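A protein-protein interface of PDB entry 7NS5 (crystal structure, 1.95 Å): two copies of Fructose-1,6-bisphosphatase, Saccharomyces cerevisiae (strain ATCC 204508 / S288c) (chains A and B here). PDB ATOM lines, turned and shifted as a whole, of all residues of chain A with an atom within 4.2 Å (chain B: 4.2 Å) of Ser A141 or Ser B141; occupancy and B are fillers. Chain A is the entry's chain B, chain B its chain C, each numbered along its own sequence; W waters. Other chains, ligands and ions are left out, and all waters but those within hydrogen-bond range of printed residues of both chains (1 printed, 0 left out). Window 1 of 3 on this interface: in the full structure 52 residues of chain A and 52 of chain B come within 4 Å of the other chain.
Water W1 bridges OG of Ser A141 and OG of Ser B141.
Ser B141 touches Val A140.
Ser A141 touches Val B140.
Ser A141 touches Ser B141.
Val A140 touches Ser B141, and with the chains exchanged Ser A141 touches Val B140.
Ser A141 touches its own counterpart, Ser B141.
Gly B178 touches its own counterpart, Gly A178.
Positions printed for both chains: 135, 140, 141, 142, 176, 177, 178, 259 and 262.
Of the 4 pairs that touch across the chains among the printed residues, 4 have their exchanged pair printed and touching as well.
The backbone carbonyl oxygen (O) of Ser A141 sits at hydrogen-bond distance from the side-chain hydroxyl (OG) of Ser A259 (2.5 Å).
N of Gly A178 sits at hydrogen-bond distance from SD of Met A176, at 3.4 Å.
The backbone carbonyl oxygen (O) of Ser B141 lies within hydrogen-bond range of the side-chain hydroxyl (OG) of Ser B259 (2.7 Å).
The side-chain sulfur of Met B176 is in hydrogen-bond range of the backbone NH of Gly B178 (3.3 Å).
The backbone carbonyl oxygen of Gly A178 sits close to the backbone carbonyl oxygen of Gly B178.
Printed residues of chain B within 4 Å of Val A140: Ser B141.
Printed residues of chain B within 4 Å of Ser A141: Val B140 and Ser B141.
Of the printed residues of chain B, Gly A178 touches Gly B178 (3.1 Å).
Of the printed residues of chain A, Val B140 touches Ser A141.
Ser B141 touches two residues of chain A.
Val B142 touches none of the printed residues of chain A.
The nearest printed residue of chain A that does not touch Ser B141 is Gly A178 (5.4 Å).
The nearest printed residue of chain A that does not touch Val B140 is Ala A262 (4.02 Å).
Of the 9 printed residues of chain A, 3 touch a printed residue of chain B.
Hydrophobic or aromatic side chains of chain A within 4 Å of the printed part of chain B: Val A140.
Of the 9 printed residues of chain B, 3 touch a printed residue of chain A.
Along chain B the printed residues that touch a printed residue of chain A span positions 140 to 178.
Among the printed residues, no Asp or Glu carboxylate lies within 4 Å of a Lys or Arg side-chain nitrogen of the other chain.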
ATOM      1  N   ASN A 135      29.420   4.954  -4.083  1.00  0.00           N
ATOM      2  CA  ASN A 135      27.996   5.151  -3.860  1.00  0.00           C
ATOM      3  C   ASN A 135      27.209   5.449  -5.138  1.00  0.00           C
ATOM      4  O   ASN A 135      25.974   5.537  -5.082  1.00  0.00           O
ATOM      5  CB  ASN A 135      27.794   6.285  -2.845  1.00  0.00           C
ATOM      6  CG  ASN A 135      27.841   5.791  -1.395  1.00  0.00           C
ATOM      7  OD1 ASN A 135      27.414   4.667  -1.091  1.00  0.00           O
ATOM      8  ND2 ASN A 135      28.313   6.647  -0.489  1.00  0.00           N
ATOM      9  N   VAL A 140      22.927   7.379  -4.204  1.00  0.00           N
ATOM     10  CA  VAL A 140      22.936   8.223  -2.983  1.00  0.00           C
ATOM     11  C   VAL A 140      23.843   9.430  -3.215  1.00  0.00           C
ATOM     12  O   VAL A 140      24.281   9.634  -4.351  1.00  0.00           O
ATOM     13  CB  VAL A 140      23.263   7.426  -1.704  1.00  0.00           C
ATOM     14  CG1 VAL A 140      22.150   6.448  -1.364  1.00  0.00           C
ATOM     15  CG2 VAL A 140      24.589   6.707  -1.802  1.00  0.00           C
ATOM     16  N   SER A 141      24.141  10.176  -2.162  1.00  0.00           N
ATOM     17  CA  SER A 141      24.880  11.429  -2.334  1.00  0.00           C
ATOM     18  C   SER A 141      26.355  11.192  -2.635  1.00  0.00           C
ATOM     19  O   SER A 141      26.978  10.277  -2.088  1.00  0.00           O
ATOM     20  CB  SER A 141      24.757  12.302  -1.081  1.00  0.00           C
ATOM     21  OG  SER A 141      23.398  12.565  -0.786  1.00  0.00           O
ATOM     22  N   VAL A 142      26.916  12.048  -3.496  1.00  0.00           N
ATOM     23  CA  VAL A 142      28.334  12.022  -3.869  1.00  0.00           C
ATOM     24  C   VAL A 142      28.743  13.482  -4.022  1.00  0.00           C
ATOM     25  O   VAL A 142      27.954  14.369  -3.734  1.00  0.00           O
ATOM     26  CB  VAL A 142      28.604  11.206  -5.155  1.00  0.00           C
ATOM     27  CG1 VAL A 142      28.284   9.684  -4.950  1.00  0.00           C
ATOM     28  CG2 VAL A 142      27.798  11.751  -6.327  1.00  0.00           C
ATOM     29  N   MET A 176      28.106  19.171  -3.455  1.00  0.00           N
ATOM     30  CA  MET A 176      27.502  17.984  -2.878  1.00  0.00           C
ATOM     31  C   MET A 176      26.292  17.662  -3.739  1.00  0.00           C
ATOM     32  O   MET A 176      25.339  18.444  -3.788  1.00  0.00           O
ATOM     33  CB  MET A 176      27.109  18.248  -1.423  1.00  0.00           C
ATOM     34  CG  MET A 176      26.843  16.989  -0.568  1.00  0.00           C
ATOM     35  SD  MET A 176      25.334  16.107  -1.035  1.00  0.00           S
ATOM     36  CE  MET A 176      24.101  17.289  -0.483  1.00  0.00           C
ATOM     37  N   TYR A 177      26.351  16.542  -4.466  1.00  0.00           N
ATOM     38  CA  TYR A 177      25.237  16.101  -5.299  1.00  0.00           C
ATOM     39  C   TYR A 177      24.396  15.149  -4.446  1.00  0.00           C
ATOM     40  O   TYR A 177      24.712  13.951  -4.320  1.00  0.00           O
ATOM     41  CB  TYR A 177      25.758  15.451  -6.574  1.00  0.00           C
ATOM     42  CG  TYR A 177      26.875  16.256  -7.226  1.00  0.00           C
ATOM     43  CD1 TYR A 177      26.626  17.526  -7.768  1.00  0.00           C
ATOM     44  CD2 TYR A 177      28.179  15.755  -7.284  1.00  0.00           C
ATOM     45  CE1 TYR A 177      27.656  18.272  -8.393  1.00  0.00           C
ATOM     46  CE2 TYR A 177      29.212  16.488  -7.879  1.00  0.00           C
ATOM     47  CZ  TYR A 177      28.945  17.739  -8.437  1.00  0.00           C
ATOM     48  OH  TYR A 177      29.989  18.434  -9.018  1.00  0.00           O
ATOM     49  N   GLY A 178      23.356  15.704  -3.808  1.00  0.00           N
ATOM     50  CA  GLY A 178      22.421  14.917  -3.021  1.00  0.00           C
ATOM     51  C   GLY A 178      21.009  14.978  -3.564  1.00  0.00           C
ATOM     52  O   GLY A 178      20.796  15.155  -4.772  1.00  0.00           O
ATOM     53  N   SER A 259      30.165   8.619   1.504  1.00  0.00           N
ATOM     54  CA  SER A 259      30.688   9.624   0.578  1.00  0.00           C
ATOM     55  C   SER A 259      31.207  10.764   1.441  1.00  0.00           C
ATOM     56  O   SER A 259      30.412  11.490   2.061  1.00  0.00           O
ATOM     57  CB  SER A 259      29.613  10.157  -0.380  1.00  0.00           C
ATOM     58  OG  SER A 259      29.099   9.164  -1.257  1.00  0.00           O
ATOM     59  N   ALA A 262      29.465  14.134   1.377  1.00  0.00           N
ATOM     60  CA  ALA A 262      28.123  14.232   1.945  1.00  0.00           C
ATOM     61  C   ALA A 262      28.185  14.188   3.462  1.00  0.00           C
ATOM     62  O   ALA A 262      27.492  14.952   4.149  1.00  0.00           O
ATOM     63  CB  ALA A 262      27.242  13.111   1.396  1.00  0.00           C
ATOM     64  N   ASN B 135      17.364  14.131   7.650  1.00  0.00           N
ATOM     65  CA  ASN B 135      18.400  14.358   6.639  1.00  0.00           C
ATOM     66  C   ASN B 135      18.071  15.492   5.659  1.00  0.00           C
ATOM     67  O   ASN B 135      18.960  15.923   4.902  1.00  0.00           O
ATOM     68  CB  ASN B 135      18.651  13.065   5.853  1.00  0.00           C
ATOM     69  CG  ASN B 135      19.690  12.180   6.511  1.00  0.00           C
ATOM     70  OD1 ASN B 135      20.600  12.682   7.175  1.00  0.00           O
ATOM     71  ND2 ASN B 135      19.574  10.861   6.316  1.00  0.00           N
ATOM     72  N   VAL B 140      20.777  15.358   1.801  1.00  0.00           N
ATOM     73  CA  VAL B 140      21.189  13.975   1.459  1.00  0.00           C
ATOM     74  C   VAL B 140      19.962  13.172   1.026  1.00  0.00           C
ATOM     75  O   VAL B 140      18.888  13.760   0.919  1.00  0.00           O
ATOM     76  CB  VAL B 140      22.052  13.319   2.550  1.00  0.00           C
ATOM     77  CG1 VAL B 140      23.465  13.875   2.534  1.00  0.00           C
ATOM     78  CG2 VAL B 140      21.444  13.489   3.924  1.00  0.00           C
ATOM     79  N   SER B 141      20.116  11.871   0.830  1.00  0.00           N
ATOM     80  CA  SER B 141      19.031  11.080   0.261  1.00  0.00           C
ATOM     81  C   SER B 141      17.890  10.893   1.262  1.00  0.00           C
ATOM     82  O   SER B 141      18.109  10.652   2.458  1.00  0.00           O
ATOM     83  CB  SER B 141      19.565   9.728  -0.185  1.00  0.00           C
ATOM     84  OG  SER B 141      20.629   9.934  -1.103  1.00  0.00           O
ATOM     85  N   VAL B 142      16.666  10.999   0.763  1.00  0.00           N
ATOM     86  CA  VAL B 142      15.470  10.744   1.567  1.00  0.00           C
ATOM     87  C   VAL B 142      14.540   9.929   0.679  1.00  0.00           C
ATOM     88  O   VAL B 142      14.956   9.503  -0.397  1.00  0.00           O
ATOM     89  CB  VAL B 142      14.807  12.048   2.065  1.00  0.00           C
ATOM     90  CG1 VAL B 142      15.724  12.786   3.065  1.00  0.00           C
ATOM     91  CG2 VAL B 142      14.411  12.950   0.877  1.00  0.00           C
ATOM     92  N   MET B 176      13.256   6.756  -3.984  1.00  0.00           N
ATOM     93  CA  MET B 176      14.442   7.096  -3.223  1.00  0.00           C
ATOM     94  C   MET B 176      14.940   8.379  -3.911  1.00  0.00           C
ATOM     95  O   MET B 176      15.292   8.357  -5.099  1.00  0.00           O
ATOM     96  CB  MET B 176      15.498   6.001  -3.278  1.00  0.00           C
ATOM     97  CG  MET B 176      16.706   6.360  -2.426  1.00  0.00           C
ATOM     98  SD  MET B 176      17.866   7.514  -3.055  1.00  0.00           S
ATOM     99  CE  MET B 176      18.712   6.580  -4.348  1.00  0.00           C
ATOM    100  N   TYR B 177      14.890   9.507  -3.199  1.00  0.00           N
ATOM    101  CA  TYR B 177      15.325  10.812  -3.704  1.00  0.00           C
ATOM    102  C   TYR B 177      16.776  11.001  -3.290  1.00  0.00           C
ATOM    103  O   TYR B 177      17.072  11.468  -2.173  1.00  0.00           O
ATOM    104  CB  TYR B 177      14.446  11.930  -3.139  1.00  0.00           C
ATOM    105  CG  TYR B 177      12.972  11.654  -3.231  1.00  0.00           C
ATOM    106  CD1 TYR B 177      12.347  11.548  -4.465  1.00  0.00           C
ATOM    107  CD2 TYR B 177      12.213  11.496  -2.099  1.00  0.00           C
ATOM    108  CE1 TYR B 177      10.991  11.293  -4.566  1.00  0.00           C
ATOM    109  CE2 TYR B 177      10.844  11.210  -2.180  1.00  0.00           C
ATOM    110  CZ  TYR B 177      10.248  11.106  -3.424  1.00  0.00           C
ATOM    111  OH  TYR B 177       8.900  10.824  -3.511  1.00  0.00           O
ATOM    112  N   GLY B 178      17.689  10.612  -4.180  1.00  0.00           N
ATOM    113  CA  GLY B 178      19.100  10.815  -3.928  1.00  0.00           C
ATOM    114  C   GLY B 178      19.723  11.718  -4.977  1.00  0.00           C
ATOM    115  O   GLY B 178      19.057  12.638  -5.472  1.00  0.00           O
ATOM    116  N   SER B 259      18.721   7.695   6.536  1.00  0.00           N
ATOM    117  CA  SER B 259      17.403   7.703   5.912  1.00  0.00           C
ATOM    118  C   SER B 259      17.134   6.273   5.509  1.00  0.00           C
ATOM    119  O   SER B 259      17.863   5.724   4.676  1.00  0.00           O
ATOM    120  CB  SER B 259      17.355   8.598   4.669  1.00  0.00           C
ATOM    121  OG  SER B 259      17.558   9.951   5.020  1.00  0.00           O
ATOM    122  N   ALA B 262      17.004   5.164   1.767  1.00  0.00           N
ATOM    123  CA  ALA B 262      18.286   5.199   1.072  1.00  0.00           C
ATOM    124  C   ALA B 262      19.151   4.003   1.450  1.00  0.00           C
ATOM    125  O   ALA B 262      19.759   3.362   0.581  1.00  0.00           O
ATOM    126  CB  ALA B 262      19.024   6.496   1.397  1.00  0.00           C
HETATM  127  O   HOH W   1      22.887  10.135   0.842  1.00  0.00           O
